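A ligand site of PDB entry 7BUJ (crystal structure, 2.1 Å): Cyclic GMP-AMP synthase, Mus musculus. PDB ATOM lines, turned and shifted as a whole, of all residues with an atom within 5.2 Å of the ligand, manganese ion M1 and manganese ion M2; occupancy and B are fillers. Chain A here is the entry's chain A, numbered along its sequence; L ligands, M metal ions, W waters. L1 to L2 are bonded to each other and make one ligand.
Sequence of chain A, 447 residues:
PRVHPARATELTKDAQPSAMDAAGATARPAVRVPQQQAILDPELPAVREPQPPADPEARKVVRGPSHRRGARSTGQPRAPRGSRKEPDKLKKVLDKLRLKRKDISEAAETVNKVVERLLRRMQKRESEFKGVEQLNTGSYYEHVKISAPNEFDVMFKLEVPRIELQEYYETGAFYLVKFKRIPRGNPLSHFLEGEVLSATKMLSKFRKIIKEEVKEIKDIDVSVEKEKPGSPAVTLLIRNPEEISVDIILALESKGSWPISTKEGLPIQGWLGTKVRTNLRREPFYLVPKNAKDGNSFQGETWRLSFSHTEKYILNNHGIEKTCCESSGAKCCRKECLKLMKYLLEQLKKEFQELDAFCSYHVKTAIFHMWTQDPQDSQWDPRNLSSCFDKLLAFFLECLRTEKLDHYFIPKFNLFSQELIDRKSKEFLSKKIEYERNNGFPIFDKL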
ATOM      1  N   GLU A 151      31.361  27.158   0.923  1.00  0.00           N
ATOM      2  CA  GLU A 151      30.684  26.506   2.029  1.00  0.00           C
ATOM      3  C   GLU A 151      29.759  25.423   1.496  1.00  0.00           C
ATOM      4  O   GLU A 151      29.272  25.505   0.375  1.00  0.00           O
ATOM      5  CB  GLU A 151      29.913  27.534   2.869  1.00  0.00           C
ATOM      6  CG  GLU A 151      30.841  28.490   3.617  1.00  0.00           C
ATOM      7  CD  GLU A 151      30.098  29.562   4.409  1.00  0.00           C
ATOM      8  OE1 GLU A 151      29.047  29.249   5.008  1.00  0.00           O
ATOM      9  OE2 GLU A 151      30.584  30.718   4.425  1.00  0.00           O
ATOM     10  N   ASP A 153      26.938  22.006   3.021  1.00  0.00           N
ATOM     11  CA  ASP A 153      26.282  21.432   4.176  1.00  0.00           C
ATOM     12  C   ASP A 153      25.717  20.074   3.804  1.00  0.00           C
ATOM     13  O   ASP A 153      25.313  19.857   2.652  1.00  0.00           O
ATOM     14  CB  ASP A 153      25.162  22.362   4.697  1.00  0.00           C
ATOM     15  CG  ASP A 153      24.139  22.674   3.633  1.00  0.00           C
ATOM     16  OD1 ASP A 153      24.397  23.574   2.785  1.00  0.00           O
ATOM     17  OD2 ASP A 153      23.090  22.031   3.615  1.00  0.00           O
ATOM     18  N   MET A 155      23.168  16.837   5.638  1.00  0.00           N
ATOM     19  CA  MET A 155      22.244  16.511   6.698  1.00  0.00           C
ATOM     20  C   MET A 155      22.332  15.026   6.953  1.00  0.00           C
ATOM     21  O   MET A 155      22.317  14.232   6.017  1.00  0.00           O
ATOM     22  CB  MET A 155      20.833  16.962   6.341  1.00  0.00           C
ATOM     23  CG  MET A 155      20.761  18.469   6.088  1.00  0.00           C
ATOM     24  SD  MET A 155      19.114  19.150   5.721  1.00  0.00           S
ATOM     25  CE  MET A 155      18.214  18.738   7.203  1.00  0.00           C
ATOM     26  N   LYS A 228      29.276  27.229  17.875  1.00  0.00           N
ATOM     27  CA  LYS A 228      28.462  28.429  17.930  1.00  0.00           C
ATOM     28  C   LYS A 228      27.200  28.151  18.733  1.00  0.00           C
ATOM     29  O   LYS A 228      26.547  27.117  18.489  1.00  0.00           O
ATOM     30  CB  LYS A 228      28.107  28.878  16.521  1.00  0.00           C
ATOM     31  CG  LYS A 228      27.501  30.268  16.447  1.00  0.00           C
ATOM     32  CD  LYS A 228      26.787  30.488  15.129  1.00  0.00           C
ATOM     33  CE  LYS A 228      26.398  31.930  14.955  1.00  0.00           C
ATOM     34  NZ  LYS A 228      27.022  32.539  13.748  1.00  0.00           N
ATOM     35  N   PRO A 229      26.804  29.011  19.666  1.00  0.00           N
ATOM     36  CA  PRO A 229      25.603  28.732  20.471  1.00  0.00           C
ATOM     37  C   PRO A 229      24.336  28.814  19.627  1.00  0.00           C
ATOM     38  O   PRO A 229      24.190  29.697  18.784  1.00  0.00           O
ATOM     39  CB  PRO A 229      25.628  29.824  21.540  1.00  0.00           C
ATOM     40  CG  PRO A 229      26.424  30.927  20.942  1.00  0.00           C
ATOM     41  CD  PRO A 229      27.476  30.254  20.090  1.00  0.00           C
ATOM     42  N   GLY A 230      23.428  27.865  19.864  1.00  0.00           N
ATOM     43  CA  GLY A 230      22.167  27.805  19.141  1.00  0.00           C
ATOM     44  C   GLY A 230      22.254  27.225  17.745  1.00  0.00           C
ATOM     45  O   GLY A 230      21.243  26.740  17.237  1.00  0.00           O
ATOM     46  N   SER A 231      23.434  27.257  17.111  1.00  0.00           N
ATOM     47  CA  SER A 231      23.605  26.746  15.765  1.00  0.00           C
ATOM     48  C   SER A 231      23.277  25.254  15.703  1.00  0.00           C
ATOM     49  O   SER A 231      23.541  24.516  16.654  1.00  0.00           O
ATOM     50  CB  SER A 231      25.044  26.958  15.299  1.00  0.00           C
ATOM     51  OG  SER A 231      25.395  26.057  14.253  1.00  0.00           O
ATOM     52  N   PRO A 232      22.696  24.794  14.597  1.00  0.00           N
ATOM     53  CA  PRO A 232      22.382  23.366  14.470  1.00  0.00           C
ATOM     54  C   PRO A 232      23.478  22.511  13.841  1.00  0.00           C
ATOM     55  O   PRO A 232      23.271  21.305  13.662  1.00  0.00           O
ATOM     56  CB  PRO A 232      21.155  23.406  13.544  1.00  0.00           C
ATOM     57  CG  PRO A 232      21.462  24.562  12.626  1.00  0.00           C
ATOM     58  CD  PRO A 232      22.203  25.576  13.456  1.00  0.00           C
ATOM     59  N   ALA A 233      24.629  23.092  13.522  1.00  0.00           N
ATOM     60  CA  ALA A 233      25.658  22.415  12.743  1.00  0.00           C
ATOM     61  C   ALA A 233      26.871  22.076  13.598  1.00  0.00           C
ATOM     62  O   ALA A 233      27.156  22.717  14.612  1.00  0.00           O
ATOM     63  CB  ALA A 233      26.135  23.291  11.571  1.00  0.00           C
ATOM     64  N   ASP A 247      29.064  22.071   6.794  1.00  0.00           N
ATOM     65  CA  ASP A 247      28.198  21.925   7.945  1.00  0.00           C
ATOM     66  C   ASP A 247      27.569  20.532   7.912  1.00  0.00           C
ATOM     67  O   ASP A 247      26.951  20.161   6.915  1.00  0.00           O
ATOM     68  CB  ASP A 247      27.114  23.000   7.933  1.00  0.00           C
ATOM     69  CG  ASP A 247      27.653  24.369   8.269  1.00  0.00           C
ATOM     70  OD1 ASP A 247      28.753  24.456   8.852  1.00  0.00           O
ATOM     71  OD2 ASP A 247      26.954  25.362   7.955  1.00  0.00           O
ATOM     72  N   ILE A 249      24.657  18.604   9.600  1.00  0.00           N
ATOM     73  CA  ILE A 249      23.451  18.947  10.362  1.00  0.00           C
ATOM     74  C   ILE A 249      22.667  17.673  10.639  1.00  0.00           C
ATOM     75  O   ILE A 249      22.144  17.039   9.716  1.00  0.00           O
ATOM     76  CB  ILE A 249      22.584  19.987   9.649  1.00  0.00           C
ATOM     77  CG1 ILE A 249      23.422  21.241   9.362  1.00  0.00           C
ATOM     78  CG2 ILE A 249      21.324  20.322  10.467  1.00  0.00           C
ATOM     79  CD1 ILE A 249      22.850  22.079   8.238  1.00  0.00           C
ATOM     80  N   VAL A 288      15.794  19.834  12.817  1.00  0.00           N
ATOM     81  CA  VAL A 288      17.216  20.075  13.099  1.00  0.00           C
ATOM     82  C   VAL A 288      17.330  20.810  14.432  1.00  0.00           C
ATOM     83  O   VAL A 288      16.395  21.511  14.847  1.00  0.00           O
ATOM     84  CB  VAL A 288      17.910  20.838  11.956  1.00  0.00           C
ATOM     85  CG1 VAL A 288      17.806  20.059  10.646  1.00  0.00           C
ATOM     86  CG2 VAL A 288      17.350  22.226  11.815  1.00  0.00           C
ATOM     87  N   LYS A 290      18.126  23.579  15.761  1.00  0.00           N
ATOM     88  CA  LYS A 290      18.216  25.040  15.838  1.00  0.00           C
ATOM     89  C   LYS A 290      17.303  25.528  16.953  1.00  0.00           C
ATOM     90  O   LYS A 290      16.074  25.443  16.853  1.00  0.00           O
ATOM     91  CB  LYS A 290      17.821  25.693  14.514  1.00  0.00           C
ATOM     92  CG  LYS A 290      17.975  27.208  14.509  1.00  0.00           C
ATOM     93  CD  LYS A 290      19.428  27.587  14.736  1.00  0.00           C
ATOM     94  CE  LYS A 290      19.618  29.072  14.947  1.00  0.00           C
ATOM     95  NZ  LYS A 290      18.959  29.847  13.875  1.00  0.00           N
ATOM     96  N   LYS A 293      14.702  31.654  19.555  1.00  0.00           N
ATOM     97  CA  LYS A 293      15.174  32.842  20.239  1.00  0.00           C
ATOM     98  C   LYS A 293      14.034  33.693  20.721  1.00  0.00           C
ATOM     99  O   LYS A 293      13.359  34.383  19.965  1.00  0.00           O
ATOM    100  CB  LYS A 293      16.076  33.659  19.354  1.00  0.00           C
ATOM    101  CG  LYS A 293      15.702  33.559  17.889  1.00  0.00           C
ATOM    102  CD  LYS A 293      16.093  32.214  17.283  1.00  0.00           C
ATOM    103  CE  LYS A 293      15.227  31.891  16.119  1.00  0.00           C
ATOM    104  NZ  LYS A 293      16.043  31.286  15.050  1.00  0.00           N
ATOM    105  N   ARG A 304      13.887  22.823  15.019  1.00  0.00           N
ATOM    106  CA  ARG A 304      13.290  23.590  13.929  1.00  0.00           C
ATOM    107  C   ARG A 304      12.993  22.698  12.737  1.00  0.00           C
ATOM    108  O   ARG A 304      13.777  21.796  12.393  1.00  0.00           O
ATOM    109  CB  ARG A 304      14.223  24.750  13.495  1.00  0.00           C
ATOM    110  CG  ARG A 304      13.520  25.954  12.887  1.00  0.00           C
ATOM    111  CD  ARG A 304      14.384  26.647  11.785  1.00  0.00           C
ATOM    112  NE  ARG A 304      14.584  25.709  10.691  1.00  0.00           N
ATOM    113  CZ  ARG A 304      15.765  25.351  10.183  1.00  0.00           C
ATOM    114  NH1 ARG A 304      16.891  25.905  10.637  1.00  0.00           N
ATOM    115  NH2 ARG A 304      15.809  24.438   9.213  1.00  0.00           N
ATOM    116  N   LEU A 305      11.828  22.947  12.108  1.00  0.00           N
ATOM    117  CA  LEU A 305      11.467  22.224  10.888  1.00  0.00           C
ATOM    118  C   LEU A 305      12.466  22.500   9.771  1.00  0.00           C
ATOM    119  O   LEU A 305      13.044  23.590   9.655  1.00  0.00           O
ATOM    120  CB  LEU A 305      10.069  22.603  10.417  1.00  0.00           C
ATOM    121  CG  LEU A 305       8.916  22.238  11.357  1.00  0.00           C
ATOM    122  CD1 LEU A 305       7.581  22.801  10.824  1.00  0.00           C
ATOM    123  CD2 LEU A 305       8.830  20.733  11.558  1.00  0.00           C
ATOM    124  N   SER A 306      12.674  21.481   8.929  1.00  0.00           N
ATOM    125  CA  SER A 306      13.513  21.657   7.755  1.00  0.00           C
ATOM    126  C   SER A 306      12.887  20.910   6.604  1.00  0.00           C
ATOM    127  O   SER A 306      12.466  19.766   6.765  1.00  0.00           O
ATOM    128  CB  SER A 306      14.947  21.135   8.008  1.00  0.00           C
ATOM    129  OG  SER A 306      15.627  20.968   6.764  1.00  0.00           O
ATOM    130  N   PHE A 307      12.852  21.524   5.445  1.00  0.00           N
ATOM    131  CA  PHE A 307      12.355  20.835   4.256  1.00  0.00           C
ATOM    132  C   PHE A 307      13.433  20.801   3.166  1.00  0.00           C
ATOM    133  O   PHE A 307      13.146  20.876   1.980  1.00  0.00           O
ATOM    134  CB  PHE A 307      11.044  21.465   3.780  1.00  0.00           C
ATOM    135  CG  PHE A 307       9.964  21.500   4.860  1.00  0.00           C
ATOM    136  CD1 PHE A 307       9.891  22.534   5.749  1.00  0.00           C
ATOM    137  CD2 PHE A 307       9.088  20.447   5.017  1.00  0.00           C
ATOM    138  CE1 PHE A 307       8.909  22.565   6.766  1.00  0.00           C
ATOM    139  CE2 PHE A 307       8.120  20.450   6.028  1.00  0.00           C
ATOM    140  CZ  PHE A 307       8.049  21.517   6.901  1.00  0.00           C
ATOM    141  N   SER A 308      14.709  20.662   3.554  1.00  0.00           N
ATOM    142  CA  SER A 308      15.792  20.707   2.556  1.00  0.00           C
ATOM    143  C   SER A 308      15.628  19.644   1.477  1.00  0.00           C
ATOM    144  O   SER A 308      15.966  19.880   0.311  1.00  0.00           O
ATOM    145  CB  SER A 308      17.147  20.563   3.238  1.00  0.00           C
ATOM    146  OG  SER A 308      17.315  21.558   4.236  1.00  0.00           O
ATOM    147  N   GLU A 311      13.063  20.989  -0.873  1.00  0.00           N
ATOM    148  CA  GLU A 311      13.684  22.077  -1.625  1.00  0.00           C
ATOM    149  C   GLU A 311      14.569  21.558  -2.771  1.00  0.00           C
ATOM    150  O   GLU A 311      14.549  22.107  -3.890  1.00  0.00           O
ATOM    151  CB  GLU A 311      14.469  22.974  -0.664  1.00  0.00           C
ATOM    152  CG  GLU A 311      13.515  23.718   0.289  1.00  0.00           C
ATOM    153  CD  GLU A 311      14.200  24.288   1.520  1.00  0.00           C
ATOM    154  OE1 GLU A 311      13.471  24.645   2.492  1.00  0.00           O
ATOM    155  OE2 GLU A 311      15.447  24.383   1.507  1.00  0.00           O
ATOM    156  N   CYS A 359      21.330  35.799   4.783  1.00  0.00           N
ATOM    157  CA  CYS A 359      21.931  34.522   4.477  1.00  0.00           C
ATOM    158  C   CYS A 359      21.362  33.959   3.192  1.00  0.00           C
ATOM    159  O   CYS A 359      20.398  34.470   2.607  1.00  0.00           O
ATOM    160  CB  CYS A 359      21.748  33.533   5.628  1.00  0.00           C
ATOM    161  SG  CYS A 359      20.022  33.090   5.964  1.00  0.00           S
ATOM    162  N   SER A 360      22.032  32.893   2.736  1.00  0.00           N
ATOM    163  CA  SER A 360      21.635  32.078   1.598  1.00  0.00           C
ATOM    164  C   SER A 360      20.138  31.711   1.571  1.00  0.00           C
ATOM    165  O   SER A 360      19.490  31.764   0.527  1.00  0.00           O
ATOM    166  CB  SER A 360      22.489  30.818   1.631  1.00  0.00           C
ATOM    167  OG  SER A 360      21.962  29.853   0.782  1.00  0.00           O
ATOM    168  N   TYR A 361      19.588  31.271   2.703  1.00  0.00           N
ATOM    169  CA  TYR A 361      18.204  30.788   2.687  1.00  0.00           C
ATOM    170  C   TYR A 361      17.203  31.913   2.449  1.00  0.00           C
ATOM    171  O   TYR A 361      16.088  31.638   1.993  1.00  0.00           O
ATOM    172  CB  TYR A 361      17.867  30.056   3.995  1.00  0.00           C
ATOM    173  CG  TYR A 361      16.590  29.216   3.885  1.00  0.00           C
ATOM    174  CD1 TYR A 361      16.558  28.042   3.120  1.00  0.00           C
ATOM    175  CD2 TYR A 361      15.423  29.617   4.519  1.00  0.00           C
ATOM    176  CE1 TYR A 361      15.361  27.266   3.009  1.00  0.00           C
ATOM    177  CE2 TYR A 361      14.244  28.871   4.430  1.00  0.00           C
ATOM    178  CZ  TYR A 361      14.221  27.707   3.676  1.00  0.00           C
ATOM    179  OH  TYR A 361      13.024  26.992   3.574  1.00  0.00           O
ATOM    180  N   HIS A 362      17.590  33.177   2.706  1.00  0.00           N
ATOM    181  CA  HIS A 362      16.740  34.322   2.381  1.00  0.00           C
ATOM    182  C   HIS A 362      16.573  34.468   0.876  1.00  0.00           C
ATOM    183  O   HIS A 362      15.451  34.661   0.376  1.00  0.00           O
ATOM    184  CB  HIS A 362      17.328  35.606   2.974  1.00  0.00           C
ATOM    185  CG  HIS A 362      17.340  35.640   4.473  1.00  0.00           C
ATOM    186  ND1 HIS A 362      18.401  36.129   5.199  1.00  0.00           N
ATOM    187  CD2 HIS A 362      16.401  35.256   5.374  1.00  0.00           C
ATOM    188  CE1 HIS A 362      18.120  36.036   6.491  1.00  0.00           C
ATOM    189  NE2 HIS A 362      16.921  35.508   6.619  1.00  0.00           N
ATOM    190  N   HIS A 407       8.519  32.218   5.349  1.00  0.00           N
ATOM    191  CA  HIS A 407       8.974  30.861   5.069  1.00  0.00           C
ATOM    192  C   HIS A 407       8.065  30.221   4.038  1.00  0.00           C
ATOM    193  O   HIS A 407       6.838  30.288   4.143  1.00  0.00           O
ATOM    194  CB  HIS A 407       9.010  30.030   6.360  1.00  0.00           C
ATOM    195  CG  HIS A 407       9.865  28.802   6.255  1.00  0.00           C
ATOM    196  ND1 HIS A 407       9.482  27.682   5.560  1.00  0.00           N
ATOM    197  CD2 HIS A 407      11.102  28.537   6.751  1.00  0.00           C
ATOM    198  CE1 HIS A 407      10.431  26.768   5.641  1.00  0.00           C
ATOM    199  NE2 HIS A 407      11.429  27.259   6.356  1.00  0.00           N
ATOM    200  N   PHE A 413       5.838  32.072   9.686  1.00  0.00           N
ATOM    201  CA  PHE A 413       7.209  32.316  10.087  1.00  0.00           C
ATOM    202  C   PHE A 413       7.792  33.331   9.115  1.00  0.00           C
ATOM    203  O   PHE A 413       7.993  33.022   7.938  1.00  0.00           O
ATOM    204  CB  PHE A 413       7.987  30.999  10.079  1.00  0.00           C
ATOM    205  CG  PHE A 413       9.395  31.089  10.576  1.00  0.00           C
ATOM    206  CD1 PHE A 413       9.766  32.012  11.528  1.00  0.00           C
ATOM    207  CD2 PHE A 413      10.354  30.218  10.092  1.00  0.00           C
ATOM    208  CE1 PHE A 413      11.091  32.086  11.981  1.00  0.00           C
ATOM    209  CE2 PHE A 413      11.672  30.279  10.554  1.00  0.00           C
ATOM    210  CZ  PHE A 413      12.039  31.223  11.500  1.00  0.00           C
ATOM    211  N   LEU A 415      10.793  35.450   7.983  1.00  0.00           N
ATOM    212  CA  LEU A 415      12.241  35.472   8.128  1.00  0.00           C
ATOM    213  C   LEU A 415      12.775  36.887   8.176  1.00  0.00           C
ATOM    214  O   LEU A 415      13.895  37.096   8.663  1.00  0.00           O
ATOM    215  CB  LEU A 415      12.890  34.723   6.957  1.00  0.00           C
ATOM    216  CG  LEU A 415      12.461  33.268   6.759  1.00  0.00           C
ATOM    217  CD1 LEU A 415      12.967  32.770   5.416  1.00  0.00           C
ATOM    218  CD2 LEU A 415      12.979  32.407   7.906  1.00  0.00           C
HETATM  219  P1  LIG L   1      21.606  32.318  12.805  1.00  0.00           P
HETATM  220  O1  LIG L   1      21.958  31.098  13.657  1.00  0.00           O
HETATM  221  O2  LIG L   1      20.102  32.497  12.888  1.00  0.00           O
HETATM  222  O3  LIG L   1      22.282  33.522  13.416  1.00  0.00           O
HETATM  223  O4  LIG L   1      22.133  32.089  11.224  1.00  0.00           O
HETATM  224  P2  LIG L   1      23.632  31.541  10.692  1.00  0.00           P
HETATM  225  O5  LIG L   1      23.822  32.018   9.284  1.00  0.00           O
HETATM  226  O6  LIG L   1      24.749  31.972  11.577  1.00  0.00           O
HETATM  227  O7  LIG L   1      23.615  29.853  10.635  1.00  0.00           O
HETATM  228  P3  LIG L   1      22.614  28.839  11.494  1.00  0.00           P
HETATM  229  O8  LIG L   1      21.201  29.306  11.476  1.00  0.00           O
HETATM  230  O9  LIG L   1      23.071  28.750  12.943  1.00  0.00           O
HETATM  231  O10 LIG L   1      22.801  27.354  10.842  1.00  0.00           O
HETATM  232  C1  LIG L   1      24.160  27.001  10.609  1.00  0.00           C
HETATM  233  C2  LIG L   1      24.319  26.617   9.162  1.00  0.00           C
HETATM  234  O11 LIG L   1      23.561  25.606   8.924  1.00  0.00           O
HETATM  235  C3  LIG L   1      23.815  27.906   8.237  1.00  0.00           C
HETATM  236  O12 LIG L   1      24.694  28.067   7.138  1.00  0.00           O
HETATM  237  C4  LIG L   1      22.531  27.606   7.889  1.00  0.00           C
HETATM  238  O13 LIG L   1      22.130  28.134   6.578  1.00  0.00           O
HETATM  239  C5  LIG L   1      22.447  26.079   7.853  1.00  0.00           C
HETATM  240  N1  LIG L   1      21.234  25.603   8.153  1.00  0.00           N
HETATM  241  C6  LIG L   1      20.405  25.969   9.159  1.00  0.00           C
HETATM  242  N2  LIG L   1      19.266  25.220   9.065  1.00  0.00           N
HETATM  243  C7  LIG L   1      19.383  24.418   8.000  1.00  0.00           C
HETATM  244  C8  LIG L   1      18.444  23.360   7.361  1.00  0.00           C
HETATM  245  O14 LIG L   1      17.338  23.112   7.823  1.00  0.00           O
HETATM  246  N3  LIG L   1      18.880  22.658   6.191  1.00  0.00           N
HETATM  247  C9  LIG L   1      20.166  22.924   5.618  1.00  0.00           C
HETATM  248  N4  LIG L   1      20.622  22.210   4.413  1.00  0.00           N
HETATM  249  N5  LIG L   1      21.029  23.934   6.219  1.00  0.00           N
HETATM  250  C10 LIG L   1      20.591  24.669   7.435  1.00  0.00           C
HETATM  251  P1  LG2 L   2      21.999  29.644   6.251  1.00  0.00           P
HETATM  252  O1  LG2 L   2      23.343  30.343   6.476  1.00  0.00           O
HETATM  253  O2  LG2 L   2      21.468  29.947   4.863  1.00  0.00           O
HETATM  254  O3  LG2 L   2      20.944  30.368   7.284  1.00  0.00           O
HETATM  255  C1  LG2 L   2      19.643  29.889   7.391  1.00  0.00           C
HETATM  256  C2  LG2 L   2      19.029  30.738   8.481  1.00  0.00           C
HETATM  257  O4  LG2 L   2      17.444  30.727   8.201  1.00  0.00           O
HETATM  258  C3  LG2 L   2      19.200  30.167   9.640  1.00  0.00           C
HETATM  259  O5  LG2 L   2      18.992  31.161  10.764  1.00  0.00           O
HETATM  260  C4  LG2 L   2      18.089  29.142   9.636  1.00  0.00           C
HETATM  261  O6  LG2 L   2      17.806  28.577  10.860  1.00  0.00           O
HETATM  262  C5  LG2 L   2      16.931  30.054   9.162  1.00  0.00           C
HETATM  263  N1  LG2 L   2      15.881  29.141   8.719  1.00  0.00           N
HETATM  264  C6  LG2 L   2      14.603  29.110   9.182  1.00  0.00           C
HETATM  265  N2  LG2 L   2      13.975  28.091   8.562  1.00  0.00           N
HETATM  266  C7  LG2 L   2      14.831  27.504   7.745  1.00  0.00           C
HETATM  267  C8  LG2 L   2      14.668  26.293   6.818  1.00  0.00           C
HETATM  268  O7  LG2 L   2      13.630  25.717   6.716  1.00  0.00           O
HETATM  269  N3  LG2 L   2      15.795  25.876   6.054  1.00  0.00           N
HETATM  270  C9  LG2 L   2      17.060  26.559   6.174  1.00  0.00           C
HETATM  271  N4  LG2 L   2      18.171  26.101   5.386  1.00  0.00           N
HETATM  272  N5  LG2 L   2      17.213  27.700   7.072  1.00  0.00           N
HETATM  273  C10 LG2 L   2      16.041  28.148   7.856  1.00  0.00           C
HETATM  274 MN    MN M   1      24.232  30.383  13.679  1.00  0.00          MN
HETATM  275 MN    MN M   2      25.975  30.634  10.202  1.00  0.00          MN
HETATM  276  O   HOH W   1      20.122  22.168   1.273  1.00  0.00           O
HETATM  277  O   HOH W   2      17.566  24.249   3.290  1.00  0.00           O
HETATM  278  O   HOH W   3      22.121  25.428   3.648  1.00  0.00           O
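Water W2 lies within hydrogen-bond range of the side-chain carboxylate (OE2) of Glu 311, a nitrogen (N4) of LG2 L2 and the side-chain hydroxyl (OG) of Ser 308. Water W3 lies within hydrogen-bond range of OD1 of Asp 153 and N5 of LIG L1.
O2 of LIG L1 is in salt-bridge range of NZ of Lys 290 (3.1 Å). SD of Met 155 sits at hydrogen-bond distance from N3 of LIG L1. An oxygen (O2) of LG2 L2 is in hydrogen-bond range of the backbone NH (N) of Tyr 361 (3.2 Å). O3 of LG2 L2 is in hydrogen-bond range of SG of Cys 359, at 3.2 Å. OH of Tyr 361 lies within hydrogen-bond range of O7 of LG2 L2, 3.4 Å away. An oxygen (O7) of LG2 L2 sits at hydrogen-bond distance from a ring nitrogen (NE2) of His 407. NZ of Lys 228 lies close to O6 of LIG L1 (3.2 Å). OG of Ser 308 lies within hydrogen-bond range of N3 of LIG L1 (2.7 Å). OG of Ser 306 sits at hydrogen-bond distance from O14 of LIG L1, at 2.9 Å. NH2 of Arg 304 is in hydrogen-bond range of O14 of LIG L1 (2.5 Å). A nitrogen (N4) of LIG L1 sits at hydrogen-bond distance from the side-chain carboxylate (OD2) of Asp 153 (2.6 Å).
Merely in contact with the ligand: Ser 231 (3.5 Å), Pro 232 (3.2 Å), Asp 247 (3.2 Å), Ile 249 (3.3 Å), Leu 305 (3.7 Å), Ser 360 (3.5 Å), Phe 413 (3.4 Å) and Leu 415 (3.9 Å). Hydrophobic or aromatic side chains within 4 Å of the ligand: Met 155, Pro 232, Ile 249, Tyr 361, His 407, Phe 413 and Leu 415. Of the 27 residues printed, 18 come within 4 Å of the ligand.
No residue comes within 4 Å of manganese ion M2.
Manganese ion M1 is bound by O9 of LIG L1 (2.1 Å), O1 of LIG L1 (2.4 Å) and O6 of LIG L1 (2.7 Å). Manganese ion M1 has three donor atoms within binding distance.
An oxygen (O6) of LIG L1 binds manganese ion M2. O7 of LIG L1 binds manganese ion M2 (2.5 Å). Slightly farther from manganese ion M2 lies O5 of LIG L1 (2.7 Å).
A ring nitrogen (NE2) of His 407 lies within hydrogen-bond range of the side-chain hydroxyl of Tyr 361 (3.2 Å). The side-chain hydroxyl (OH) of Tyr 361 lies within hydrogen-bond range of the side-chain carboxylate (OE1) of Glu 311. The side-chain sulfur (SG) of Cys 359 lies close to the backbone NH (N) of Tyr 361, 3.8 Å away. The backbone NH (N) of His 407 sits at hydrogen-bond distance from the backbone carbonyl oxygen (O) of Phe 413 (2.8 Å). N of Cys 359 sits at hydrogen-bond distance from ND1 of His 362, at 3.0 Å. OG of Ser 308 sits at hydrogen-bond distance from SD of Met 155, 3.4 Å away. The backbone carbonyl oxygen (O) of Val 288 is in hydrogen-bond range of the backbone NH (N) of Arg 304, at 2.8 Å. The backbone NH (N) of Ala 233 lies within hydrogen-bond range of the side-chain hydroxyl (OG) of Ser 231, 3.1 Å away.
Merely in contact with manganese ion M1: Lys 228 (2.9 Å) and Ser 231 (3.9 Å). Along chain A the residues within 4 Å of manganese ion M1 span positions 228 to 231. The nearest printed residue that does not touch manganese ion M1 is Lys 290 (5.0 Å).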
